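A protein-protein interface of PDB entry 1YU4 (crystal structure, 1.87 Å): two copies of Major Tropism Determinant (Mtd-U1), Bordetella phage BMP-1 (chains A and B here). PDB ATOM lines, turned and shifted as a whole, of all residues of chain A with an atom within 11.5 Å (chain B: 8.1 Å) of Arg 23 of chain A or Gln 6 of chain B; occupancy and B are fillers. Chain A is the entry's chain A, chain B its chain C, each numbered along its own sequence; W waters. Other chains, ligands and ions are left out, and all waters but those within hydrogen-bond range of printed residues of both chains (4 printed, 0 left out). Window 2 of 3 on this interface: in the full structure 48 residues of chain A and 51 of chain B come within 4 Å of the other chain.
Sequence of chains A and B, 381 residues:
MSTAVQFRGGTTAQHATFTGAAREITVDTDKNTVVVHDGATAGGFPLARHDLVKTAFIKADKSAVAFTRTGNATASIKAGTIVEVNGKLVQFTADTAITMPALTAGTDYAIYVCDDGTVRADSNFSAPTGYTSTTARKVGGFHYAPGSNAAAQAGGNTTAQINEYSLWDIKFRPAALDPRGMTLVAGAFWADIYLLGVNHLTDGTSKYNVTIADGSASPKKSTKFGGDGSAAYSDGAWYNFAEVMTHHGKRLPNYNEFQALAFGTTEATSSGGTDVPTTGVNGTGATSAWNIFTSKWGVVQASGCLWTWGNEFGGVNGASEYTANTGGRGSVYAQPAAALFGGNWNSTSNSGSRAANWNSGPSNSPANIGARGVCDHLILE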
ATOM      1  N   GLN A   6       8.310  -3.352  21.606  1.00  0.00           N
ATOM      2  CA  GLN A   6       8.466  -3.136  23.042  1.00  0.00           C
ATOM      3  C   GLN A   6       7.796  -1.824  23.441  1.00  0.00           C
ATOM      4  O   GLN A   6       7.701  -0.902  22.640  1.00  0.00           O
ATOM      5  CB  GLN A   6       9.948  -3.114  23.411  1.00  0.00           C
ATOM      6  CG  GLN A   6      10.665  -4.414  23.092  1.00  0.00           C
ATOM      7  CD  GLN A   6      12.164  -4.326  23.295  1.00  0.00           C
ATOM      8  OE1 GLN A   6      12.642  -4.230  24.425  1.00  0.00           O
ATOM      9  NE2 GLN A   6      12.911  -4.364  22.203  1.00  0.00           N
ATOM     10  N   PHE A   7       7.342  -1.743  24.686  1.00  0.00           N
ATOM     11  CA  PHE A   7       6.581  -0.592  25.162  1.00  0.00           C
ATOM     12  C   PHE A   7       7.462   0.282  26.032  1.00  0.00           C
ATOM     13  O   PHE A   7       8.483  -0.174  26.540  1.00  0.00           O
ATOM     14  CB  PHE A   7       5.369  -1.054  25.968  1.00  0.00           C
ATOM     15  CG  PHE A   7       4.170  -1.377  25.131  1.00  0.00           C
ATOM     16  CD1 PHE A   7       2.968  -0.721  25.349  1.00  0.00           C
ATOM     17  CD2 PHE A   7       4.234  -2.340  24.135  1.00  0.00           C
ATOM     18  CE1 PHE A   7       1.851  -1.015  24.589  1.00  0.00           C
ATOM     19  CE2 PHE A   7       3.118  -2.638  23.367  1.00  0.00           C
ATOM     20  CZ  PHE A   7       1.925  -1.971  23.598  1.00  0.00           C
ATOM     21  N   ARG A   8       7.062   1.541  26.197  1.00  0.00           N
ATOM     22  CA  ARG A   8       7.758   2.453  27.100  1.00  0.00           C
ATOM     23  C   ARG A   8       7.616   1.907  28.514  1.00  0.00           C
ATOM     24  O   ARG A   8       6.513   1.573  28.940  1.00  0.00           O
ATOM     25  CB  ARG A   8       7.175   3.869  27.018  1.00  0.00           C
ATOM     26  CG  ARG A   8       8.107   4.968  27.545  1.00  0.00           C
ATOM     27  CD  ARG A   8       8.654   5.910  26.461  1.00  0.00           C
ATOM     28  NE  ARG A   8       9.991   6.433  26.774  1.00  0.00           N
ATOM     29  CZ  ARG A   8      11.140   5.773  26.595  1.00  0.00           C
ATOM     30  NH1 ARG A   8      11.151   4.537  26.100  1.00  0.00           N
ATOM     31  NH2 ARG A   8      12.293   6.354  26.921  1.00  0.00           N
ATOM     32  N   PHE A  18       5.536  10.089  37.178  1.00  0.00           N
ATOM     33  CA  PHE A  18       5.135  10.107  35.773  1.00  0.00           C
ATOM     34  C   PHE A  18       3.624  10.269  35.576  1.00  0.00           C
ATOM     35  O   PHE A  18       2.840   9.367  35.886  1.00  0.00           O
ATOM     36  CB  PHE A  18       5.614   8.828  35.073  1.00  0.00           C
ATOM     37  CG  PHE A  18       5.384   8.825  33.586  1.00  0.00           C
ATOM     38  CD1 PHE A  18       6.146   9.636  32.751  1.00  0.00           C
ATOM     39  CD2 PHE A  18       4.402   8.017  33.021  1.00  0.00           C
ATOM     40  CE1 PHE A  18       5.934   9.640  31.374  1.00  0.00           C
ATOM     41  CE2 PHE A  18       4.184   8.016  31.644  1.00  0.00           C
ATOM     42  CZ  PHE A  18       4.952   8.829  30.820  1.00  0.00           C
ATOM     43  N   THR A  19       3.236  11.435  35.067  1.00  0.00           N
ATOM     44  CA  THR A  19       1.892  11.674  34.564  1.00  0.00           C
ATOM     45  C   THR A  19       1.997  11.675  33.045  1.00  0.00           C
ATOM     46  O   THR A  19       2.415  12.673  32.451  1.00  0.00           O
ATOM     47  CB  THR A  19       1.367  13.035  35.060  1.00  0.00           C
ATOM     48  OG1 THR A  19       1.175  12.999  36.480  1.00  0.00           O
ATOM     49  CG2 THR A  19      -0.022  13.325  34.507  1.00  0.00           C
ATOM     50  N   GLY A  20       1.634  10.561  32.418  1.00  0.00           N
ATOM     51  CA  GLY A  20       1.804  10.408  30.982  1.00  0.00           C
ATOM     52  C   GLY A  20       0.808  11.219  30.172  1.00  0.00           C
ATOM     53  O   GLY A  20       0.560  12.391  30.458  1.00  0.00           O
ATOM     54  N   ALA A  21       0.252  10.593  29.140  1.00  0.00           N
ATOM     55  CA  ALA A  21      -0.840  11.172  28.367  1.00  0.00           C
ATOM     56  C   ALA A  21      -2.065  10.280  28.515  1.00  0.00           C
ATOM     57  O   ALA A  21      -1.976   9.177  29.058  1.00  0.00           O
ATOM     58  CB  ALA A  21      -0.447  11.296  26.904  1.00  0.00           C
ATOM     59  N   ALA A  22      -3.207  10.757  28.029  1.00  0.00           N
ATOM     60  CA  ALA A  22      -4.438   9.981  28.068  1.00  0.00           C
ATOM     61  C   ALA A  22      -4.299   8.764  27.160  1.00  0.00           C
ATOM     62  O   ALA A  22      -3.760   8.864  26.058  1.00  0.00           O
ATOM     63  CB  ALA A  22      -5.622  10.834  27.643  1.00  0.00           C
ATOM     64  N   ARG A  23      -4.771   7.618  27.645  1.00  0.00           N
ATOM     65  CA  ARG A  23      -4.738   6.357  26.903  1.00  0.00           C
ATOM     66  C   ARG A  23      -3.328   5.819  26.627  1.00  0.00           C
ATOM     67  O   ARG A  23      -3.157   4.968  25.762  1.00  0.00           O
ATOM     68  CB  ARG A  23      -5.524   6.479  25.588  1.00  0.00           C
ATOM     69  CG  ARG A  23      -6.899   7.124  25.738  1.00  0.00           C
ATOM     70  CD  ARG A  23      -7.628   7.366  24.423  1.00  0.00           C
ATOM     71  NE  ARG A  23      -6.850   8.182  23.490  1.00  0.00           N
ATOM     72  CZ  ARG A  23      -6.681   9.499  23.585  1.00  0.00           C
ATOM     73  NH1 ARG A  23      -7.220  10.195  24.586  1.00  0.00           N
ATOM     74  NH2 ARG A  23      -5.956  10.131  22.668  1.00  0.00           N
ATOM     75  N   GLU A  24      -2.327   6.288  27.369  1.00  0.00           N
ATOM     76  CA  GLU A  24      -0.978   5.740  27.251  1.00  0.00           C
ATOM     77  C   GLU A  24      -0.889   4.449  28.063  1.00  0.00           C
ATOM     78  O   GLU A  24      -1.365   4.386  29.192  1.00  0.00           O
ATOM     79  CB  GLU A  24       0.084   6.735  27.735  1.00  0.00           C
ATOM     80  CG  GLU A  24       1.519   6.262  27.498  1.00  0.00           C
ATOM     81  CD  GLU A  24       2.582   7.226  28.000  1.00  0.00           C
ATOM     82  OE1 GLU A  24       2.230   8.297  28.534  1.00  0.00           O
ATOM     83  OE2 GLU A  24       3.786   6.908  27.861  1.00  0.00           O
ATOM     84  N   ILE A  25      -0.290   3.423  27.473  1.00  0.00           N
ATOM     85  CA  ILE A  25      -0.034   2.161  28.154  1.00  0.00           C
ATOM     86  C   ILE A  25       1.476   1.994  28.309  1.00  0.00           C
ATOM     87  O   ILE A  25       2.203   2.009  27.319  1.00  0.00           O
ATOM     88  CB  ILE A  25      -0.634   0.994  27.337  1.00  0.00           C
ATOM     89  CG1 ILE A  25      -2.162   1.002  27.446  1.00  0.00           C
ATOM     90  CG2 ILE A  25      -0.066  -0.345  27.797  1.00  0.00           C
ATOM     91  CD1 ILE A  25      -2.863   0.159  26.393  1.00  0.00           C
ATOM     92  N   THR A  26       1.939   1.849  29.549  1.00  0.00           N
ATOM     93  CA  THR A  26       3.350   1.594  29.836  1.00  0.00           C
ATOM     94  C   THR A  26       3.512   0.273  30.579  1.00  0.00           C
ATOM     95  O   THR A  26       2.530  -0.356  30.962  1.00  0.00           O
ATOM     96  CB  THR A  26       3.961   2.745  30.665  1.00  0.00           C
ATOM     97  OG1 THR A  26       3.181   2.979  31.847  1.00  0.00           O
ATOM     98  CG2 THR A  26       3.890   4.063  29.902  1.00  0.00           C
ATOM     99  N   VAL A  27       4.757  -0.145  30.772  1.00  0.00           N
ATOM    100  CA  VAL A  27       5.055  -1.381  31.476  1.00  0.00           C
ATOM    101  C   VAL A  27       5.927  -1.074  32.683  1.00  0.00           C
ATOM    102  O   VAL A  27       7.031  -0.543  32.543  1.00  0.00           O
ATOM    103  CB  VAL A  27       5.774  -2.398  30.565  1.00  0.00           C
ATOM    104  CG1 VAL A  27       6.255  -3.613  31.364  1.00  0.00           C
ATOM    105  CG2 VAL A  27       4.855  -2.836  29.436  1.00  0.00           C
ATOM    106  N   VAL A  34       1.062  -3.970  33.225  1.00  0.00           N
ATOM    107  CA  VAL A  34       0.721  -2.786  32.445  1.00  0.00           C
ATOM    108  C   VAL A  34       0.207  -1.695  33.378  1.00  0.00           C
ATOM    109  O   VAL A  34      -0.482  -1.984  34.351  1.00  0.00           O
ATOM    110  CB  VAL A  34      -0.363  -3.123  31.392  1.00  0.00           C
ATOM    111  CG1 VAL A  34      -0.981  -1.855  30.795  1.00  0.00           C
ATOM    112  CG2 VAL A  34       0.215  -4.017  30.304  1.00  0.00           C
ATOM    113  N   VAL A  35       0.555  -0.446  33.080  1.00  0.00           N
ATOM    114  CA  VAL A  35       0.031   0.714  33.791  1.00  0.00           C
ATOM    115  C   VAL A  35      -0.676   1.631  32.794  1.00  0.00           C
ATOM    116  O   VAL A  35      -0.044   2.161  31.882  1.00  0.00           O
ATOM    117  CB  VAL A  35       1.153   1.494  34.500  1.00  0.00           C
ATOM    118  CG1 VAL A  35       0.575   2.651  35.315  1.00  0.00           C
ATOM    119  CG2 VAL A  35       1.972   0.563  35.386  1.00  0.00           C
ATOM    120  N   VAL A  36      -1.984   1.796  32.958  1.00  0.00           N
ATOM    121  CA  VAL A  36      -2.758   2.714  32.131  1.00  0.00           C
ATOM    122  C   VAL A  36      -2.608   4.135  32.681  1.00  0.00           C
ATOM    123  O   VAL A  36      -2.558   4.328  33.894  1.00  0.00           O
ATOM    124  CB  VAL A  36      -4.254   2.312  32.095  1.00  0.00           C
ATOM    125  CG1 VAL A  36      -5.058   3.287  31.259  1.00  0.00           C
ATOM    126  CG2 VAL A  36      -4.414   0.898  31.554  1.00  0.00           C
ATOM    127  N   HIS A  37      -2.539   5.120  31.787  1.00  0.00           N
ATOM    128  CA  HIS A  37      -2.407   6.529  32.168  1.00  0.00           C
ATOM    129  C   HIS A  37      -3.586   7.344  31.646  1.00  0.00           C
ATOM    130  O   HIS A  37      -4.200   6.991  30.641  1.00  0.00           O
ATOM    131  CB  HIS A  37      -1.092   7.114  31.643  1.00  0.00           C
ATOM    132  CG  HIS A  37       0.127   6.446  32.197  1.00  0.00           C
ATOM    133  ND1 HIS A  37       0.390   6.378  33.547  1.00  0.00           N
ATOM    134  CD2 HIS A  37       1.149   5.803  31.584  1.00  0.00           C
ATOM    135  CE1 HIS A  37       1.522   5.725  33.743  1.00  0.00           C
ATOM    136  NE2 HIS A  37       2.002   5.365  32.567  1.00  0.00           N
ATOM    137  N   ASP A  38      -3.899   8.428  32.347  1.00  0.00           N
ATOM    138  CA  ASP A  38      -4.998   9.319  31.967  1.00  0.00           C
ATOM    139  C   ASP A  38      -4.532  10.755  31.706  1.00  0.00           C
ATOM    140  O   ASP A  38      -5.356  11.638  31.467  1.00  0.00           O
ATOM    141  CB  ASP A  38      -6.104   9.301  33.034  1.00  0.00           C
ATOM    142  CG  ASP A  38      -5.646   9.846  34.381  1.00  0.00           C
ATOM    143  OD1 ASP A  38      -4.426   9.928  34.620  1.00  0.00           O
ATOM    144  OD2 ASP A  38      -6.442  10.201  35.277  1.00  0.00           O
ATOM    145  N   GLY A  39      -3.219  10.980  31.747  1.00  0.00           N
ATOM    146  CA  GLY A  39      -2.647  12.294  31.519  1.00  0.00           C
ATOM    147  C   GLY A  39      -2.902  13.304  32.627  1.00  0.00           C
ATOM    148  O   GLY A  39      -2.898  14.509  32.373  1.00  0.00           O
ATOM    149  N   ALA A  40      -3.102  12.822  33.853  1.00  0.00           N
ATOM    150  CA  ALA A  40      -3.408  13.695  34.992  1.00  0.00           C
ATOM    151  C   ALA A  40      -2.947  13.102  36.329  1.00  0.00           C
ATOM    152  O   ALA A  40      -2.267  13.771  37.114  1.00  0.00           O
ATOM    153  CB  ALA A  40      -4.901  13.991  35.037  1.00  0.00           C
ATOM    154  N   THR A  41      -3.330  11.854  36.580  1.00  0.00           N
ATOM    155  CA  THR A  41      -2.983  11.160  37.817  1.00  0.00           C
ATOM    156  C   THR A  41      -1.553  10.631  37.772  1.00  0.00           C
ATOM    157  O   THR A  41      -1.222   9.799  36.927  1.00  0.00           O
ATOM    158  CB  THR A  41      -3.955   9.985  38.062  1.00  0.00           C
ATOM    159  OG1 THR A  41      -5.305  10.405  37.827  1.00  0.00           O
ATOM    160  CG2 THR A  41      -3.947   9.569  39.528  1.00  0.00           C
ATOM    161  N   GLY A  44      -0.321   6.664  37.643  1.00  0.00           N
ATOM    162  CA  GLY A  44      -1.178   5.959  36.710  1.00  0.00           C
ATOM    163  C   GLY A  44      -2.104   4.979  37.409  1.00  0.00           C
ATOM    164  O   GLY A  44      -2.524   5.209  38.546  1.00  0.00           O
ATOM    165  N   PHE A  45      -2.412   3.884  36.718  1.00  0.00           N
ATOM    166  CA  PHE A  45      -3.343   2.872  37.202  1.00  0.00           C
ATOM    167  C   PHE A  45      -2.803   1.500  36.829  1.00  0.00           C
ATOM    168  O   PHE A  45      -3.129   0.974  35.766  1.00  0.00           O
ATOM    169  CB  PHE A  45      -4.735   3.089  36.601  1.00  0.00           C
ATOM    170  CG  PHE A  45      -5.299   4.453  36.877  1.00  0.00           C
ATOM    171  CD1 PHE A  45      -5.994   4.708  38.053  1.00  0.00           C
ATOM    172  CD2 PHE A  45      -5.113   5.488  35.974  1.00  0.00           C
ATOM    173  CE1 PHE A  45      -6.506   5.967  38.317  1.00  0.00           C
ATOM    174  CE2 PHE A  45      -5.619   6.749  36.230  1.00  0.00           C
ATOM    175  CZ  PHE A  45      -6.322   6.990  37.406  1.00  0.00           C
ATOM    176  N   LEU A  47      -2.319  -2.458  36.516  1.00  0.00           N
ATOM    177  CA  LEU A  47      -3.287  -3.535  36.363  1.00  0.00           C
ATOM    178  C   LEU A  47      -2.817  -4.735  37.171  1.00  0.00           C
ATOM    179  O   LEU A  47      -1.638  -4.849  37.505  1.00  0.00           O
ATOM    180  CB  LEU A  47      -3.457  -3.920  34.890  1.00  0.00           C
ATOM    181  CG  LEU A  47      -3.868  -2.815  33.907  1.00  0.00           C
ATOM    182  CD1 LEU A  47      -4.200  -3.420  32.553  1.00  0.00           C
ATOM    183  CD2 LEU A  47      -5.040  -1.999  34.425  1.00  0.00           C
ATOM    184  N   VAL B   5       2.917   7.797  22.818  1.00  0.00           N
ATOM    185  CA  VAL B   5       1.986   6.866  22.121  1.00  0.00           C
ATOM    186  C   VAL B   5       0.707   6.689  22.933  1.00  0.00           C
ATOM    187  O   VAL B   5       0.757   6.307  24.095  1.00  0.00           O
ATOM    188  CB  VAL B   5       2.634   5.483  21.889  1.00  0.00           C
ATOM    189  CG1 VAL B   5       1.618   4.487  21.323  1.00  0.00           C
ATOM    190  CG2 VAL B   5       3.833   5.604  20.955  1.00  0.00           C
ATOM    191  N   GLN B   6      -0.429   6.982  22.309  1.00  0.00           N
ATOM    192  CA  GLN B   6      -1.742   6.776  22.911  1.00  0.00           C
ATOM    193  C   GLN B   6      -2.514   5.741  22.099  1.00  0.00           C
ATOM    194  O   GLN B   6      -2.336   5.638  20.888  1.00  0.00           O
ATOM    195  CB  GLN B   6      -2.519   8.091  22.950  1.00  0.00           C
ATOM    196  CG  GLN B   6      -1.744   9.259  23.539  1.00  0.00           C
ATOM    197  CD  GLN B   6      -2.469  10.577  23.372  1.00  0.00           C
ATOM    198  OE1 GLN B   6      -3.125  11.055  24.299  1.00  0.00           O
ATOM    199  NE2 GLN B   6      -2.353  11.167  22.190  1.00  0.00           N
ATOM    200  N   PHE B   7      -3.376   4.981  22.764  1.00  0.00           N
ATOM    201  CA  PHE B   7      -4.137   3.923  22.110  1.00  0.00           C
ATOM    202  C   PHE B   7      -5.581   4.338  21.921  1.00  0.00           C
ATOM    203  O   PHE B   7      -6.029   5.324  22.501  1.00  0.00           O
ATOM    204  CB  PHE B   7      -4.031   2.628  22.912  1.00  0.00           C
ATOM    205  CG  PHE B   7      -2.679   2.002  22.828  1.00  0.00           C
ATOM    206  CD1 PHE B   7      -2.369   1.153  21.783  1.00  0.00           C
ATOM    207  CD2 PHE B   7      -1.697   2.304  23.760  1.00  0.00           C
ATOM    208  CE1 PHE B   7      -1.110   0.589  21.682  1.00  0.00           C
ATOM    209  CE2 PHE B   7      -0.434   1.741  23.664  1.00  0.00           C
ATOM    210  CZ  PHE B   7      -0.140   0.883  22.623  1.00  0.00           C
ATOM    211  N   ARG B   8      -6.289   3.599  21.072  1.00  0.00           N
ATOM    212  CA  ARG B   8      -7.719   3.807  20.859  1.00  0.00           C
ATOM    213  C   ARG B   8      -8.426   3.711  22.205  1.00  0.00           C
ATOM    214  O   ARG B   8      -8.111   2.838  23.010  1.00  0.00           O
ATOM    215  CB  ARG B   8      -8.278   2.760  19.886  1.00  0.00           C
ATOM    216  CG  ARG B   8      -9.636   3.109  19.278  1.00  0.00           C
ATOM    217  CD  ARG B   8      -9.556   3.955  18.004  1.00  0.00           C
ATOM    218  NE  ARG B   8     -10.517   5.066  18.009  1.00  0.00           N
ATOM    219  CZ  ARG B   8     -10.207   6.367  17.931  1.00  0.00           C
ATOM    220  NH1 ARG B   8      -8.939   6.778  17.837  1.00  0.00           N
ATOM    221  NH2 ARG B   8     -11.183   7.272  17.951  1.00  0.00           N
ATOM    222  N   GLY B   9      -9.361   4.622  22.455  1.00  0.00           N
ATOM    223  CA  GLY B   9     -10.074   4.641  23.719  1.00  0.00           C
ATOM    224  C   GLY B   9     -11.465   5.232  23.650  1.00  0.00           C
ATOM    225  O   GLY B   9     -11.914   5.704  22.603  1.00  0.00           O
ATOM    226  N   GLY B  10     -12.144   5.204  24.792  1.00  0.00           N
ATOM    227  CA  GLY B  10     -13.518   5.660  24.890  1.00  0.00           C
ATOM    228  C   GLY B  10     -14.198   5.216  26.173  1.00  0.00           C
ATOM    229  O   GLY B  10     -13.686   4.363  26.900  1.00  0.00           O
ATOM    230  N   ILE B  25      -6.246  -3.982  21.408  1.00  0.00           N
ATOM    231  CA  ILE B  25      -6.291  -3.479  22.778  1.00  0.00           C
ATOM    232  C   ILE B  25      -6.768  -2.034  22.745  1.00  0.00           C
ATOM    233  O   ILE B  25      -6.223  -1.224  22.001  1.00  0.00           O
ATOM    234  CB  ILE B  25      -4.887  -3.552  23.416  1.00  0.00           C
ATOM    235  CG1 ILE B  25      -4.470  -5.011  23.620  1.00  0.00           C
ATOM    236  CG2 ILE B  25      -4.847  -2.788  24.738  1.00  0.00           C
ATOM    237  CD1 ILE B  25      -2.977  -5.196  23.833  1.00  0.00           C
ATOM    238  N   THR B  26      -7.779  -1.717  23.548  1.00  0.00           N
ATOM    239  CA  THR B  26      -8.214  -0.335  23.745  1.00  0.00           C
ATOM    240  C   THR B  26      -8.145   0.031  25.221  1.00  0.00           C
ATOM    241  O   THR B  26      -7.857  -0.809  26.066  1.00  0.00           O
ATOM    242  CB  THR B  26      -9.647  -0.122  23.224  1.00  0.00           C
ATOM    243  OG1 THR B  26     -10.557  -0.990  23.913  1.00  0.00           O
ATOM    244  CG2 THR B  26      -9.768  -0.523  21.753  1.00  0.00           C
ATOM    245  N   VAL B  27      -8.414   1.297  25.516  1.00  0.00           N
ATOM    246  CA  VAL B  27      -8.391   1.811  26.876  1.00  0.00           C
ATOM    247  C   VAL B  27      -9.777   2.343  27.214  1.00  0.00           C
ATOM    248  O   VAL B  27     -10.272   3.257  26.556  1.00  0.00           O
ATOM    249  CB  VAL B  27      -7.348   2.934  27.024  1.00  0.00           C
ATOM    250  CG1 VAL B  27      -7.464   3.623  28.382  1.00  0.00           C
ATOM    251  CG2 VAL B  27      -5.945   2.377  26.820  1.00  0.00           C
ATOM    252  N   ASP B  28     -10.411   1.741  28.216  1.00  0.00           N
ATOM    253  CA  ASP B  28     -11.621   2.292  28.807  1.00  0.00           C
ATOM    254  C   ASP B  28     -11.222   3.495  29.661  1.00  0.00           C
ATOM    255  O   ASP B  28     -10.554   3.340  30.683  1.00  0.00           O
ATOM    256  CB  ASP B  28     -12.338   1.230  29.651  1.00  0.00           C
ATOM    257  CG  ASP B  28     -13.746   1.634  30.026  1.00  0.00           C
ATOM    258  OD1 ASP B  28     -13.924   2.768  30.505  1.00  0.00           O
ATOM    259  OD2 ASP B  28     -14.737   0.890  29.879  1.00  0.00           O
ATOM    260  N   THR B  29     -11.626   4.687  29.229  1.00  0.00           N
ATOM    261  CA  THR B  29     -11.218   5.937  29.877  1.00  0.00           C
ATOM    262  C   THR B  29     -12.034   6.273  31.126  1.00  0.00           C
ATOM    263  O   THR B  29     -11.608   7.100  31.935  1.00  0.00           O
ATOM    264  CB  THR B  29     -11.297   7.120  28.884  1.00  0.00           C
ATOM    265  OG1 THR B  29     -12.606   7.183  28.302  1.00  0.00           O
ATOM    266  CG2 THR B  29     -10.362   6.909  27.700  1.00  0.00           C
ATOM    267  N   ASN B  32     -10.200   3.579  33.473  1.00  0.00           N
ATOM    268  CA  ASN B  32      -8.742   3.566  33.351  1.00  0.00           C
ATOM    269  C   ASN B  32      -8.156   2.151  33.340  1.00  0.00           C
ATOM    270  O   ASN B  32      -7.226   1.837  34.090  1.00  0.00           O
ATOM    271  CB  ASN B  32      -8.097   4.419  34.444  1.00  0.00           C
ATOM    272  CG  ASN B  32      -8.452   5.884  34.316  1.00  0.00           C
ATOM    273  OD1 ASN B  32      -9.024   6.478  35.229  1.00  0.00           O
ATOM    274  ND2 ASN B  32      -8.123   6.474  33.171  1.00  0.00           N
ATOM    275  N   THR B  33      -8.711   1.299  32.484  1.00  0.00           N
ATOM    276  CA  THR B  33      -8.171  -0.040  32.282  1.00  0.00           C
ATOM    277  C   THR B  33      -8.108  -0.415  30.800  1.00  0.00           C
ATOM    278  O   THR B  33      -8.635   0.292  29.944  1.00  0.00           O
ATOM    279  CB  THR B  33      -8.994  -1.082  33.079  1.00  0.00           C
ATOM    280  OG1 THR B  33      -8.278  -2.319  33.151  1.00  0.00           O
ATOM    281  CG2 THR B  33     -10.303  -1.438  32.370  1.00  0.00           C
ATOM    282  N   VAL B  34      -7.438  -1.527  30.522  1.00  0.00           N
ATOM    283  CA  VAL B  34      -7.330  -2.076  29.177  1.00  0.00           C
ATOM    284  C   VAL B  34      -8.517  -2.994  28.894  1.00  0.00           C
ATOM    285  O   VAL B  34      -8.987  -3.697  29.784  1.00  0.00           O
ATOM    286  CB  VAL B  34      -5.997  -2.852  29.030  1.00  0.00           C
ATOM    287  CG1 VAL B  34      -6.029  -3.829  27.850  1.00  0.00           C
ATOM    288  CG2 VAL B  34      -4.842  -1.872  28.901  1.00  0.00           C
HETATM  289  O   HOH W   1      -7.010   6.757  30.310  1.00  0.00           O
HETATM  290  O   HOH W   2      -6.125   7.657  20.500  1.00  0.00           O
HETATM  291  O   HOH W   3       1.645   3.997  25.013  1.00  0.00           O
HETATM  292  O   HOH W   4      -8.966   9.285  35.307  1.00  0.00           O
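O of Arg 23 of chain A sits at hydrogen-bond distance from N of Phe 7 of chain B (3.0 Å).
O of Ala 22 of chain A lies close to OE1 of Gln 6 of chain B (2.9 Å).
The guanidinium group (NH2) of Arg 23 of chain A sits at hydrogen-bond distance from the side-chain amide oxygen (OE1) of Gln 6 of chain B, 3.4 Å away.
O of Ala 21 of chain A sits at hydrogen-bond distance from N of Gly 39 of chain A, 3.5 Å away.
N of Gly 10 of chain B lies within hydrogen-bond range of O of Val 27 of chain B (3.2 Å).
The backbone carbonyl oxygen (O) of Val 34 of chain A is in hydrogen-bond range of the backbone NH (N) of Leu 47 of chain A (2.9 Å).
The backbone carbonyl oxygen of Glu 24 of chain A sits at hydrogen-bond distance from the backbone NH of His 37 of chain A (2.9 Å).
Among the printed residues, merely in contact across the chains: Phe 7 of chain A with Phe 7 of chain B, Ala 21 of chain A with Gln 6 of chain B, Arg 23 of chain A with Gly 9 of chain B, Arg 23 of chain A with Val 27 of chain B, Arg 23 of chain A with Thr 29 of chain B, Glu 24 of chain A with Val 5 of chain B, Ile 25 of chain A with Phe 7 of chain B, Ile 25 of chain A with Ile 25 of chain B, Ile 25 of chain A with Val 27 of chain B, Ile 25 of chain A with Val 34 of chain B, Val 36 of chain A with Val 27 of chain B, Val 36 of chain A with Asn 32 of chain B, Val 36 of chain A with Thr 33 of chain B, Val 36 of chain A with Val 34 of chain B, Asp 38 of chain A with Asn 32 of chain B, Phe 45 of chain A with Asn 32 of chain B, Leu 47 of chain A with Thr 33 of chain B and Leu 47 of chain A with Val 34 of chain B.
Of the printed residues of chain B, Ile 25 of chain A touches Phe 7 (3.6 Å), Ile 25 (3.9 Å), Val 27 (3.8 Å) and Val 34 (3.8 Å).
Gly 44 of chain A touches none of the printed residues of chain B.
Of chain A, only Glu 24 comes within 4 Å of Val 5 of chain B.
Of chain A, only Ala 21, Ala 22 and Arg 23 come within 4 Å of Gln 6 of chain B.
No residue of chain A comes within 4 Å of Arg 8 of chain B.
Gly 9 of chain B touches just one residue of chain A: Arg 23.
Thr 26 of chain B touches none of the printed residues of chain A.
Of chain A, only Arg 23, Ile 25 and Val 36 come within 4 Å of Val 27 of chain B.
Of the printed residues of chain A, Thr 29 of chain B touches Arg 23.
The nearest residue of chain A that does not touch Gln 6 of chain B is Glu 24 of chain A (4.5 Å).
Printed residues of chain A that touch a printed residue of chain B: Phe 7, Ala 21, Ala 22, Arg 23, Glu 24, Ile 25, Val 36, Asp 38, Phe 45 and Leu 47.
Along chain A the printed residues that touch a printed residue of chain B span positions 7 to 47.
Among the printed residues, no Asp or Glu carboxylate lies within 4 Å of a Lys or Arg side-chain nitrogen of the other chain.
Phe 7 of chain B touches its own counterpart, Phe 7 of chain A.
Ile 25 of chain B touches its own counterpart, Ile 25 of chain A.
Ile 25 of chain A touches Val 34 of chain B, but with the chains exchanged Val 34 of chain A does not touch Ile 25 of chain B (7.2 Å).
Positions printed for both chains: 6, 7, 8, 25, 26, 27 and 34.
Of the 21 pairs that touch across the chains among the printed residues, 2 have their exchanged pair printed and touching as well.
Water W3 bridges O of Val 5 of chain B (2.6 Å) and O of Ile 25 of chain A (3.1 Å).
Water W4 bridges OD2 of Asp 38 of chain A and OD1 of Asn 32 of chain B.
Water W1 bridges O of His 37 of chain A (2.8 Å) and ND2 of Asn 32 of chain B (3.1 Å).
Water W2 lies within hydrogen-bond range of O of Phe 7 of chain B and NE of Arg 23 of chain A.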
